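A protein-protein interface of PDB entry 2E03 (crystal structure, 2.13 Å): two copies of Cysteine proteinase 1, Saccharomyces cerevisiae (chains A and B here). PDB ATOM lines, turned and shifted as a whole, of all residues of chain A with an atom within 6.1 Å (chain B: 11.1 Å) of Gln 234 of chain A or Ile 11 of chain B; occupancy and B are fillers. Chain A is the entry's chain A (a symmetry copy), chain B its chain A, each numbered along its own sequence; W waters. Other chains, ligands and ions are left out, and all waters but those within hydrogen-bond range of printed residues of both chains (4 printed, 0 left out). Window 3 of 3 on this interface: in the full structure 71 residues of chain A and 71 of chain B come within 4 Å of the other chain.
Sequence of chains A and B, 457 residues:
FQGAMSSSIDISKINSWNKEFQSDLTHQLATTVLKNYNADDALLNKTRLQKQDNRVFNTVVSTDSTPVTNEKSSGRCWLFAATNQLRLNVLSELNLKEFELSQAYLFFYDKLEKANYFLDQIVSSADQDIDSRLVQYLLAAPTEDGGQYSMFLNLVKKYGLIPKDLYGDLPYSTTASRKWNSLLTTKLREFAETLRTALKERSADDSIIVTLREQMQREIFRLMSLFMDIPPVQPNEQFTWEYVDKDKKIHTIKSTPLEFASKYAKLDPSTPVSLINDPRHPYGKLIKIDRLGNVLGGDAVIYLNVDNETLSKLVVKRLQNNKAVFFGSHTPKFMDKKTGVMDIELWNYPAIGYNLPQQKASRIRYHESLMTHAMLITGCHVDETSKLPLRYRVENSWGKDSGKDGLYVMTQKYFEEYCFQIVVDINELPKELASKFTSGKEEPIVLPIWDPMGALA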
ATOM      1  N   TYR A 105      -2.325 -18.883 -14.063  1.00  0.00           N
ATOM      2  CA  TYR A 105      -2.233 -18.756 -15.511  1.00  0.00           C
ATOM      3  C   TYR A 105      -3.667 -18.713 -16.147  1.00  0.00           C
ATOM      4  O   TYR A 105      -4.020 -17.835 -16.970  1.00  0.00           O
ATOM      5  CB  TYR A 105      -1.437 -19.978 -16.067  1.00  0.00           C
ATOM      6  CG  TYR A 105      -1.222 -19.991 -17.560  1.00  0.00           C
ATOM      7  CD1 TYR A 105      -0.236 -19.187 -18.154  1.00  0.00           C
ATOM      8  CD2 TYR A 105      -1.951 -20.859 -18.384  1.00  0.00           C
ATOM      9  CE1 TYR A 105       0.023 -19.254 -19.570  1.00  0.00           C
ATOM     10  CE2 TYR A 105      -1.701 -20.944 -19.765  1.00  0.00           C
ATOM     11  CZ  TYR A 105      -0.705 -20.121 -20.366  1.00  0.00           C
ATOM     12  OH  TYR A 105      -0.472 -20.182 -21.741  1.00  0.00           O
ATOM     13  N   TYR A 109      -6.079 -15.249 -17.694  1.00  0.00           N
ATOM     14  CA  TYR A 109      -6.820 -15.281 -18.974  1.00  0.00           C
ATOM     15  C   TYR A 109      -8.363 -15.402 -18.830  1.00  0.00           C
ATOM     16  O   TYR A 109      -9.129 -14.863 -19.649  1.00  0.00           O
ATOM     17  CB  TYR A 109      -6.267 -16.418 -19.909  1.00  0.00           C
ATOM     18  CG  TYR A 109      -4.843 -16.131 -20.392  1.00  0.00           C
ATOM     19  CD1 TYR A 109      -4.517 -14.893 -20.972  1.00  0.00           C
ATOM     20  CD2 TYR A 109      -3.858 -17.085 -20.310  1.00  0.00           C
ATOM     21  CE1 TYR A 109      -3.195 -14.633 -21.484  1.00  0.00           C
ATOM     22  CE2 TYR A 109      -2.573 -16.856 -20.789  1.00  0.00           C
ATOM     23  CZ  TYR A 109      -2.247 -15.646 -21.380  1.00  0.00           C
ATOM     24  OH  TYR A 109      -0.994 -15.498 -21.899  1.00  0.00           O
ATOM     25  N   LYS A 158      -7.423 -22.525 -25.953  1.00  0.00           N
ATOM     26  CA  LYS A 158      -6.728 -21.368 -26.524  1.00  0.00           C
ATOM     27  C   LYS A 158      -5.351 -21.101 -25.892  1.00  0.00           C
ATOM     28  O   LYS A 158      -4.428 -20.618 -26.564  1.00  0.00           O
ATOM     29  CB  LYS A 158      -7.592 -20.098 -26.337  1.00  0.00           C
ATOM     30  CG  LYS A 158      -7.039 -18.753 -26.877  1.00  0.00           C
ATOM     31  CD  LYS A 158      -8.076 -17.585 -26.678  1.00  0.00           C
ATOM     32  CE  LYS A 158      -7.651 -16.287 -27.362  1.00  0.00           C
ATOM     33  NZ  LYS A 158      -8.771 -15.263 -27.345  1.00  0.00           N
ATOM     34  N   TYR A 159      -5.211 -21.409 -24.605  1.00  0.00           N
ATOM     35  CA  TYR A 159      -3.988 -21.058 -23.861  1.00  0.00           C
ATOM     36  C   TYR A 159      -3.081 -22.164 -23.390  1.00  0.00           C
ATOM     37  O   TYR A 159      -1.944 -21.909 -23.039  1.00  0.00           O
ATOM     38  CB  TYR A 159      -4.401 -20.208 -22.637  1.00  0.00           C
ATOM     39  CG  TYR A 159      -5.026 -18.862 -23.025  1.00  0.00           C
ATOM     40  CD1 TYR A 159      -4.224 -17.813 -23.487  1.00  0.00           C
ATOM     41  CD2 TYR A 159      -6.403 -18.655 -22.941  1.00  0.00           C
ATOM     42  CE1 TYR A 159      -4.754 -16.591 -23.851  1.00  0.00           C
ATOM     43  CE2 TYR A 159      -6.968 -17.436 -23.307  1.00  0.00           C
ATOM     44  CZ  TYR A 159      -6.124 -16.394 -23.768  1.00  0.00           C
ATOM     45  OH  TYR A 159      -6.660 -15.173 -24.128  1.00  0.00           O
ATOM     46  N   ILE A 230       1.308 -10.500 -17.389  1.00  0.00           N
ATOM     47  CA  ILE A 230       0.757 -11.397 -18.400  1.00  0.00           C
ATOM     48  C   ILE A 230       1.685 -12.638 -18.276  1.00  0.00           C
ATOM     49  O   ILE A 230       2.843 -12.498 -17.899  1.00  0.00           O
ATOM     50  CB  ILE A 230       0.886 -10.769 -19.818  1.00  0.00           C
ATOM     51  CG1 ILE A 230       0.210 -11.683 -20.844  1.00  0.00           C
ATOM     52  CG2 ILE A 230       2.379 -10.522 -20.163  1.00  0.00           C
ATOM     53  CD1 ILE A 230      -0.075 -10.991 -22.202  1.00  0.00           C
ATOM     54  N   PRO A 231       1.171 -13.868 -18.527  1.00  0.00           N
ATOM     55  CA  PRO A 231       2.095 -15.031 -18.412  1.00  0.00           C
ATOM     56  C   PRO A 231       3.378 -14.775 -19.228  1.00  0.00           C
ATOM     57  O   PRO A 231       3.363 -14.035 -20.223  1.00  0.00           O
ATOM     58  CB  PRO A 231       1.244 -16.186 -18.936  1.00  0.00           C
ATOM     59  CG  PRO A 231      -0.093 -15.835 -18.329  1.00  0.00           C
ATOM     60  CD  PRO A 231      -0.230 -14.323 -18.600  1.00  0.00           C
ATOM     61  N   PRO A 232       4.521 -15.374 -18.796  1.00  0.00           N
ATOM     62  CA  PRO A 232       5.809 -15.210 -19.436  1.00  0.00           C
ATOM     63  C   PRO A 232       5.971 -15.753 -20.871  1.00  0.00           C
ATOM     64  O   PRO A 232       6.920 -15.376 -21.510  1.00  0.00           O
ATOM     65  CB  PRO A 232       6.762 -15.878 -18.441  1.00  0.00           C
ATOM     66  CG  PRO A 232       5.973 -17.020 -17.989  1.00  0.00           C
ATOM     67  CD  PRO A 232       4.605 -16.415 -17.760  1.00  0.00           C
ATOM     68  N   VAL A 233       5.083 -16.628 -21.372  1.00  0.00           N
ATOM     69  CA  VAL A 233       5.230 -17.155 -22.763  1.00  0.00           C
ATOM     70  C   VAL A 233       3.831 -17.253 -23.320  1.00  0.00           C
ATOM     71  O   VAL A 233       2.888 -17.409 -22.534  1.00  0.00           O
ATOM     72  CB  VAL A 233       5.866 -18.622 -22.881  1.00  0.00           C
ATOM     73  CG1 VAL A 233       7.336 -18.630 -22.340  1.00  0.00           C
ATOM     74  CG2 VAL A 233       5.034 -19.628 -22.125  1.00  0.00           C
ATOM     75  N   GLN A 234       3.728 -17.060 -24.646  1.00  0.00           N
ATOM     76  CA  GLN A 234       2.504 -17.144 -25.398  1.00  0.00           C
ATOM     77  C   GLN A 234       2.170 -18.630 -25.566  1.00  0.00           C
ATOM     78  O   GLN A 234       3.042 -19.475 -25.453  1.00  0.00           O
ATOM     79  CB  GLN A 234       2.692 -16.357 -26.714  1.00  0.00           C
ATOM     80  CG  GLN A 234       2.941 -14.890 -26.348  1.00  0.00           C
ATOM     81  CD  GLN A 234       3.310 -13.979 -27.542  1.00  0.00           C
ATOM     82  OE1 GLN A 234       2.678 -14.049 -28.589  1.00  0.00           O
ATOM     83  NE2 GLN A 234       4.316 -13.133 -27.366  1.00  0.00           N
ATOM     84  N   PRO A 235       0.923 -18.972 -25.887  1.00  0.00           N
ATOM     85  CA  PRO A 235       0.513 -20.390 -25.997  1.00  0.00           C
ATOM     86  C   PRO A 235       1.246 -21.375 -26.897  1.00  0.00           C
ATOM     87  O   PRO A 235       1.310 -22.583 -26.582  1.00  0.00           O
ATOM     88  CB  PRO A 235      -0.997 -20.300 -26.312  1.00  0.00           C
ATOM     89  CG  PRO A 235      -1.383 -18.982 -25.797  1.00  0.00           C
ATOM     90  CD  PRO A 235      -0.219 -18.075 -26.143  1.00  0.00           C
ATOM     91  N   ASN A 236       1.801 -20.850 -27.998  1.00  0.00           N
ATOM     92  CA  ASN A 236       2.530 -21.648 -28.991  1.00  0.00           C
ATOM     93  C   ASN A 236       4.013 -21.343 -28.887  1.00  0.00           C
ATOM     94  O   ASN A 236       4.780 -21.775 -29.740  1.00  0.00           O
ATOM     95  CB  ASN A 236       2.047 -21.297 -30.410  1.00  0.00           C
ATOM     96  CG  ASN A 236       0.655 -21.851 -30.695  1.00  0.00           C
ATOM     97  OD1 ASN A 236       0.526 -23.008 -31.018  1.00  0.00           O
ATOM     98  ND2 ASN A 236      -0.373 -21.031 -30.540  1.00  0.00           N
ATOM     99  N   GLU A 237       4.373 -20.544 -27.893  1.00  0.00           N
ATOM    100  CA  GLU A 237       5.761 -20.192 -27.596  1.00  0.00           C
ATOM    101  C   GLU A 237       6.365 -21.206 -26.622  1.00  0.00           C
ATOM    102  O   GLU A 237       5.729 -21.619 -25.641  1.00  0.00           O
ATOM    103  CB  GLU A 237       5.841 -18.816 -26.941  1.00  0.00           C
ATOM    104  CG  GLU A 237       7.273 -18.378 -26.576  1.00  0.00           C
ATOM    105  CD  GLU A 237       7.369 -16.899 -26.080  1.00  0.00           C
ATOM    106  OE1 GLU A 237       6.337 -16.258 -25.800  1.00  0.00           O
ATOM    107  OE2 GLU A 237       8.501 -16.364 -25.976  1.00  0.00           O
ATOM    108  N   GLN A 238       7.608 -21.595 -26.865  1.00  0.00           N
ATOM    109  CA  GLN A 238       8.255 -22.544 -25.997  1.00  0.00           C
ATOM    110  C   GLN A 238       8.771 -21.948 -24.728  1.00  0.00           C
ATOM    111  O   GLN A 238       9.321 -20.852 -24.728  1.00  0.00           O
ATOM    112  CB  GLN A 238       9.502 -23.188 -26.654  1.00  0.00           C
ATOM    113  CG  GLN A 238       9.259 -24.042 -27.872  1.00  0.00           C
ATOM    114  CD  GLN A 238      10.556 -24.742 -28.336  1.00  0.00           C
ATOM    115  OE1 GLN A 238      11.577 -24.102 -28.552  1.00  0.00           O
ATOM    116  NE2 GLN A 238      10.505 -26.053 -28.455  1.00  0.00           N
ATOM    117  N   THR A 256       5.688 -25.913 -25.298  1.00  0.00           N
ATOM    118  CA  THR A 256       4.847 -24.729 -25.324  1.00  0.00           C
ATOM    119  C   THR A 256       3.677 -25.051 -24.373  1.00  0.00           C
ATOM    120  O   THR A 256       3.420 -26.216 -24.050  1.00  0.00           O
ATOM    121  CB  THR A 256       4.226 -24.509 -26.710  1.00  0.00           C
ATOM    122  OG1 THR A 256       3.279 -25.583 -26.983  1.00  0.00           O
ATOM    123  CG2 THR A 256       5.327 -24.452 -27.822  1.00  0.00           C
ATOM    124  N   PRO A 257       2.921 -24.015 -23.964  1.00  0.00           N
ATOM    125  CA  PRO A 257       1.814 -24.352 -23.063  1.00  0.00           C
ATOM    126  C   PRO A 257       0.801 -25.304 -23.725  1.00  0.00           C
ATOM    127  O   PRO A 257       0.231 -26.154 -23.064  1.00  0.00           O
ATOM    128  CB  PRO A 257       1.176 -22.982 -22.738  1.00  0.00           C
ATOM    129  CG  PRO A 257       2.402 -21.999 -22.787  1.00  0.00           C
ATOM    130  CD  PRO A 257       3.262 -22.574 -23.936  1.00  0.00           C
ATOM    131  N   ALA B   4     -16.416 -10.641 -35.217  1.00  0.00           N
ATOM    132  CA  ALA B   4     -16.109 -11.492 -34.093  1.00  0.00           C
ATOM    133  C   ALA B   4     -14.620 -11.561 -33.836  1.00  0.00           C
ATOM    134  O   ALA B   4     -14.191 -11.620 -32.688  1.00  0.00           O
ATOM    135  CB  ALA B   4     -16.650 -12.895 -34.312  1.00  0.00           C
ATOM    136  N   MET B   5     -13.849 -11.585 -34.926  1.00  0.00           N
ATOM    137  CA  MET B   5     -12.432 -11.658 -34.875  1.00  0.00           C
ATOM    138  C   MET B   5     -11.952 -10.366 -34.196  1.00  0.00           C
ATOM    139  O   MET B   5     -11.155 -10.407 -33.241  1.00  0.00           O
ATOM    140  CB  MET B   5     -11.897 -11.800 -36.318  1.00  0.00           C
ATOM    141  CG  MET B   5     -10.364 -11.802 -36.477  1.00  0.00           C
ATOM    142  SD  MET B   5      -9.723 -13.463 -36.973  1.00  0.00           S
ATOM    143  CE  MET B   5     -10.892 -14.549 -35.943  1.00  0.00           C
ATOM    144  N   SER B   6     -12.487  -9.233 -34.631  1.00  0.00           N
ATOM    145  CA  SER B   6     -12.056  -7.962 -34.083  1.00  0.00           C
ATOM    146  C   SER B   6     -12.454  -7.853 -32.637  1.00  0.00           C
ATOM    147  O   SER B   6     -11.782  -7.152 -31.845  1.00  0.00           O
ATOM    148  CB  SER B   6     -12.653  -6.721 -34.919  1.00  0.00           C
ATOM    149  N   SER B   7     -13.539  -8.539 -32.275  1.00  0.00           N
ATOM    150  CA  SER B   7     -14.023  -8.487 -30.893  1.00  0.00           C
ATOM    151  C   SER B   7     -13.310  -9.478 -29.939  1.00  0.00           C
ATOM    152  O   SER B   7     -13.531  -9.441 -28.727  1.00  0.00           O
ATOM    153  CB  SER B   7     -15.536  -8.752 -30.881  1.00  0.00           C
ATOM    154  OG  SER B   7     -16.159  -7.744 -31.650  1.00  0.00           O
ATOM    155  N   SER B   8     -12.476 -10.359 -30.488  1.00  0.00           N
ATOM    156  CA  SER B   8     -11.781 -11.335 -29.665  1.00  0.00           C
ATOM    157  C   SER B   8     -10.536 -10.775 -29.016  1.00  0.00           C
ATOM    158  O   SER B   8      -9.998  -9.721 -29.426  1.00  0.00           O
ATOM    159  CB  SER B   8     -11.370 -12.540 -30.517  1.00  0.00           C
ATOM    160  OG  SER B   8     -12.487 -13.167 -31.142  1.00  0.00           O
ATOM    161  N   ILE B   9     -10.053 -11.492 -28.002  1.00  0.00           N
ATOM    162  CA  ILE B   9      -8.806 -11.141 -27.338  1.00  0.00           C
ATOM    163  C   ILE B   9      -7.697 -11.711 -28.264  1.00  0.00           C
ATOM    164  O   ILE B   9      -7.591 -12.968 -28.545  1.00  0.00           O
ATOM    165  CB  ILE B   9      -8.682 -11.800 -25.899  1.00  0.00           C
ATOM    166  CG1 ILE B   9      -9.621 -11.072 -24.932  1.00  0.00           C
ATOM    167  CG2 ILE B   9      -7.219 -11.789 -25.440  1.00  0.00           C
ATOM    168  CD1 ILE B   9      -9.358  -9.568 -24.717  1.00  0.00           C
ATOM    169  N   ASP B  10      -6.883 -10.795 -28.772  1.00  0.00           N
ATOM    170  CA  ASP B  10      -5.847 -11.261 -29.677  1.00  0.00           C
ATOM    171  C   ASP B  10      -4.508 -11.327 -28.897  1.00  0.00           C
ATOM    172  O   ASP B  10      -4.097 -10.322 -28.332  1.00  0.00           O
ATOM    173  CB  ASP B  10      -5.712 -10.346 -30.899  1.00  0.00           C
ATOM    174  CG  ASP B  10      -4.590 -10.855 -31.840  1.00  0.00           C
ATOM    175  OD1 ASP B  10      -4.845 -11.838 -32.596  1.00  0.00           O
ATOM    176  OD2 ASP B  10      -3.447 -10.326 -31.757  1.00  0.00           O
ATOM    177  N   ILE B  11      -3.840 -12.489 -28.902  1.00  0.00           N
ATOM    178  CA  ILE B  11      -2.597 -12.657 -28.122  1.00  0.00           C
ATOM    179  C   ILE B  11      -1.458 -11.749 -28.550  1.00  0.00           C
ATOM    180  O   ILE B  11      -0.712 -11.271 -27.705  1.00  0.00           O
ATOM    181  CB  ILE B  11      -2.176 -14.135 -28.091  1.00  0.00           C
ATOM    182  CG1 ILE B  11      -3.324 -14.886 -27.397  1.00  0.00           C
ATOM    183  CG2 ILE B  11      -0.835 -14.362 -27.272  1.00  0.00           C
ATOM    184  CD1 ILE B  11      -3.271 -16.371 -27.536  1.00  0.00           C
ATOM    185  N   SER B  12      -1.314 -11.508 -29.854  1.00  0.00           N
ATOM    186  CA  SER B  12      -0.268 -10.597 -30.310  1.00  0.00           C
ATOM    187  C   SER B  12      -0.531  -9.181 -29.770  1.00  0.00           C
ATOM    188  O   SER B  12       0.403  -8.521 -29.330  1.00  0.00           O
ATOM    189  CB  SER B  12      -0.179 -10.521 -31.874  1.00  0.00           C
ATOM    190  OG  SER B  12       0.751  -9.467 -32.226  1.00  0.00           O
ATOM    191  N   LYS B  13      -1.780  -8.717 -29.837  1.00  0.00           N
ATOM    192  CA  LYS B  13      -2.141  -7.374 -29.363  1.00  0.00           C
ATOM    193  C   LYS B  13      -1.823  -7.176 -27.884  1.00  0.00           C
ATOM    194  O   LYS B  13      -1.243  -6.182 -27.505  1.00  0.00           O
ATOM    195  CB  LYS B  13      -3.653  -7.083 -29.489  1.00  0.00           C
ATOM    196  CG  LYS B  13      -4.218  -7.132 -30.909  1.00  0.00           C
ATOM    197  CD  LYS B  13      -5.627  -6.527 -30.989  1.00  0.00           C
ATOM    198  CE  LYS B  13      -6.106  -6.654 -32.428  1.00  0.00           C
ATOM    199  NZ  LYS B  13      -7.229  -5.786 -32.713  1.00  0.00           N
ATOM    200  N   ILE B  14      -2.241  -8.116 -27.040  1.00  0.00           N
ATOM    201  CA  ILE B  14      -2.017  -7.891 -25.602  1.00  0.00           C
ATOM    202  C   ILE B  14      -0.542  -7.935 -25.244  1.00  0.00           C
ATOM    203  O   ILE B  14      -0.110  -7.206 -24.369  1.00  0.00           O
ATOM    204  CB  ILE B  14      -2.874  -8.899 -24.688  1.00  0.00           C
ATOM    205  CG1 ILE B  14      -2.422 -10.343 -24.931  1.00  0.00           C
ATOM    206  CG2 ILE B  14      -4.426  -8.642 -24.980  1.00  0.00           C
ATOM    207  CD1 ILE B  14      -3.124 -11.398 -24.017  1.00  0.00           C
ATOM    208  N   ASN B  15       0.225  -8.762 -25.943  1.00  0.00           N
ATOM    209  CA  ASN B  15       1.643  -8.847 -25.673  1.00  0.00           C
ATOM    210  C   ASN B  15       2.360  -7.580 -26.221  1.00  0.00           C
ATOM    211  O   ASN B  15       3.324  -7.080 -25.604  1.00  0.00           O
ATOM    212  CB  ASN B  15       2.164 -10.164 -26.294  1.00  0.00           C
ATOM    213  CG  ASN B  15       1.989 -11.321 -25.342  1.00  0.00           C
ATOM    214  OD1 ASN B  15       2.801 -11.476 -24.469  1.00  0.00           O
ATOM    215  ND2 ASN B  15       0.913 -12.121 -25.492  1.00  0.00           N
ATOM    216  N   SER B  16       1.842  -7.016 -27.320  1.00  0.00           N
ATOM    217  CA  SER B  16       2.443  -5.794 -27.875  1.00  0.00           C
ATOM    218  C   SER B  16       2.071  -4.613 -26.968  1.00  0.00           C
ATOM    219  O   SER B  16       2.902  -3.746 -26.654  1.00  0.00           O
ATOM    220  CB  SER B  16       1.910  -5.567 -29.304  1.00  0.00           C
ATOM    221  OG  SER B  16       2.207  -6.700 -30.115  1.00  0.00           O
ATOM    222  N   TRP B  17       0.841  -4.610 -26.489  1.00  0.00           N
ATOM    223  CA  TRP B  17       0.417  -3.555 -25.583  1.00  0.00           C
ATOM    224  C   TRP B  17       1.265  -3.689 -24.295  1.00  0.00           C
ATOM    225  O   TRP B  17       1.726  -2.701 -23.700  1.00  0.00           O
ATOM    226  CB  TRP B  17      -1.069  -3.729 -25.245  1.00  0.00           C
ATOM    227  CG  TRP B  17      -1.988  -3.389 -26.325  1.00  0.00           C
ATOM    228  CD1 TRP B  17      -1.740  -2.540 -27.415  1.00  0.00           C
ATOM    229  CD2 TRP B  17      -3.353  -3.838 -26.475  1.00  0.00           C
ATOM    230  NE1 TRP B  17      -2.861  -2.469 -28.205  1.00  0.00           N
ATOM    231  CE2 TRP B  17      -3.862  -3.243 -27.659  1.00  0.00           C
ATOM    232  CE3 TRP B  17      -4.191  -4.669 -25.717  1.00  0.00           C
ATOM    233  CZ2 TRP B  17      -5.189  -3.463 -28.112  1.00  0.00           C
ATOM    234  CZ3 TRP B  17      -5.516  -4.892 -26.158  1.00  0.00           C
ATOM    235  CH2 TRP B  17      -5.997  -4.289 -27.353  1.00  0.00           C
ATOM    236  N   ASN B  18       1.429  -4.915 -23.839  1.00  0.00           N
ATOM    237  CA  ASN B  18       2.223  -5.141 -22.640  1.00  0.00           C
ATOM    238  C   ASN B  18       3.636  -4.544 -22.847  1.00  0.00           C
ATOM    239  O   ASN B  18       4.153  -3.882 -21.953  1.00  0.00           O
ATOM    240  CB  ASN B  18       2.417  -6.633 -22.331  1.00  0.00           C
ATOM    241  CG  ASN B  18       3.121  -6.828 -20.967  1.00  0.00           C
ATOM    242  OD1 ASN B  18       2.672  -6.287 -19.971  1.00  0.00           O
ATOM    243  ND2 ASN B  18       4.237  -7.529 -20.947  1.00  0.00           N
ATOM    244  N   LYS B  19       4.262  -4.800 -24.007  1.00  0.00           N
ATOM    245  CA  LYS B  19       5.606  -4.239 -24.278  1.00  0.00           C
ATOM    246  C   LYS B  19       5.556  -2.688 -24.192  1.00  0.00           C
ATOM    247  O   LYS B  19       6.442  -2.047 -23.596  1.00  0.00           O
ATOM    248  CB  LYS B  19       6.110  -4.694 -25.652  1.00  0.00           C
ATOM    249  CG  LYS B  19       7.443  -4.133 -26.078  1.00  0.00           C
ATOM    250  CD  LYS B  19       7.962  -4.949 -27.276  1.00  0.00           C
ATOM    251  CE  LYS B  19       8.957  -4.195 -28.169  1.00  0.00           C
ATOM    252  NZ  LYS B  19      10.243  -4.155 -27.519  1.00  0.00           N
ATOM    253  N   GLU B  20       4.534  -2.080 -24.774  1.00  0.00           N
ATOM    254  CA  GLU B  20       4.398  -0.638 -24.720  1.00  0.00           C
ATOM    255  C   GLU B  20       4.236  -0.142 -23.243  1.00  0.00           C
ATOM    256  O   GLU B  20       4.942   0.757 -22.776  1.00  0.00           O
ATOM    257  CB  GLU B  20       3.195  -0.212 -25.544  1.00  0.00           C
ATOM    258  CG  GLU B  20       3.023   1.288 -25.414  1.00  0.00           C
ATOM    259  CD  GLU B  20       1.988   1.853 -26.328  1.00  0.00           C
ATOM    260  OE1 GLU B  20       1.795   1.328 -27.445  1.00  0.00           O
ATOM    261  OE2 GLU B  20       1.360   2.848 -25.948  1.00  0.00           O
HETATM  262  O   HOH W   1     -11.349 -13.860 -27.259  1.00  0.00           O
HETATM  263  O   HOH W   2       3.332 -13.829 -22.854  1.00  0.00           O
HETATM  264  O   HOH W   3       2.438  -7.872 -17.867  1.00  0.00           O
HETATM  265  O   HOH W   4       0.597 -14.308 -23.797  1.00  0.00           O
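Of the 17 printed residues of chain B, 5 touch a printed residue of chain A. Hydrophobic or aromatic side chains of chain B that line the printed part of chain A: Ile 9, Ile 11 and Ile 14. Printed residues of chain A that touch a printed residue of chain B: Lys 158, Tyr 159, Ile 230, Gln 234 and Pro 235. Hydrophobic or aromatic side chains of chain A that line the printed part of chain B: Tyr 159, Ile 230 and Pro 235. Among the printed residues, no Asp or Glu carboxylate lies within 4 Å of a Lys or Arg side-chain nitrogen of the other chain.
Water W2 lies within hydrogen-bond range of O of Pro 231 of chain A (2.6 Å) and OD1 of Asn 15 of chain B (2.9 Å). Water W3 bridges the side-chain amide oxygen (OD1) of Asn 18 of chain B (2.6 Å) and the backbone NH (N) of Ile 230 of chain A (2.9 Å). Water W4 bridges the side-chain hydroxyl (OH) of Tyr 109 of chain A (2.7 Å) and the side-chain amide nitrogen (ND2) of Asn 15 of chain B (2.8 Å). Water W1 bridges N of Ile 9 of chain B (2.8 Å) and NZ of Lys 158 of chain A (2.9 Å).
Among the printed residues, pairs that only touch across the chains: Tyr 159 of chain A with Ile 9 of chain B, Tyr 159 of chain A with Ile 11 of chain B, Ile 230 of chain A with Ile 14 of chain B, Ile 230 of chain A with Asn 15 of chain B, Ile 230 of chain A with Asn 18 of chain B, Gln 234 of chain A with Ile 11 of chain B, Gln 234 of chain A with Asn 15 of chain B and Pro 235 of chain A with Ile 11 of chain B.
The backbone carbonyl oxygen (O) of Ile 9 of chain B sits at hydrogen-bond distance from the side-chain amino group (NZ) of Lys 158 of chain A, at 2.8 Å.
The backbone NH (N) of Gln 234 of chain A sits at hydrogen-bond distance from the side-chain carboxylate (OE1) of Glu 237 of chain A (3.0 Å). ND2 of Asn 15 of chain B lies within hydrogen-bond range of O of Ile 11 of chain B (2.9 Å). The backbone carbonyl oxygen (O) of Tyr 159 of chain A lies within hydrogen-bond range of the side-chain hydroxyl (OH) of Tyr 105 of chain A (2.6 Å).
Of chain B, only Ile 9 and Ile 11 come within 4 Å of Tyr 159 of chain A. Of the printed residues of chain B, Ile 230 of chain A touches Ile 14, Asn 15 and Asn 18. No residue of chain B comes within 4 Å of Pro 232 of chain A. No residue of chain B comes within 4 Å of Val 233 of chain A. Of chain B, only Ile 11 comes within 4 Å of Pro 235 of chain A. No residue of chain B comes within 4 Å of Thr 256 of chain A. Ile 11 of chain B touches just these residues of chain A: Tyr 159, Gln 234 and Pro 235. Printed residues of chain A within 4 Å of Ile 14 of chain B: Ile 230 (3.6 Å). Of the printed residues of chain A, Asn 15 of chain B touches Ile 230 (3.6 Å) and Gln 234 (3.5 Å). Of the printed residues of chain A, Asn 18 of chain B touches Ile 230. The nearest residue of chain B that does not touch Gln 234 of chain A is Ser 12 of chain B (4.9 Å). The nearest residue of chain A that does not touch Ile 11 of chain B is Lys 158 of chain A (4.4 Å). The nearest printed residue of chain B that does not touch Ile 230 of chain A is Ile 11 of chain B (5.5 Å).
No position is printed for both chains.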
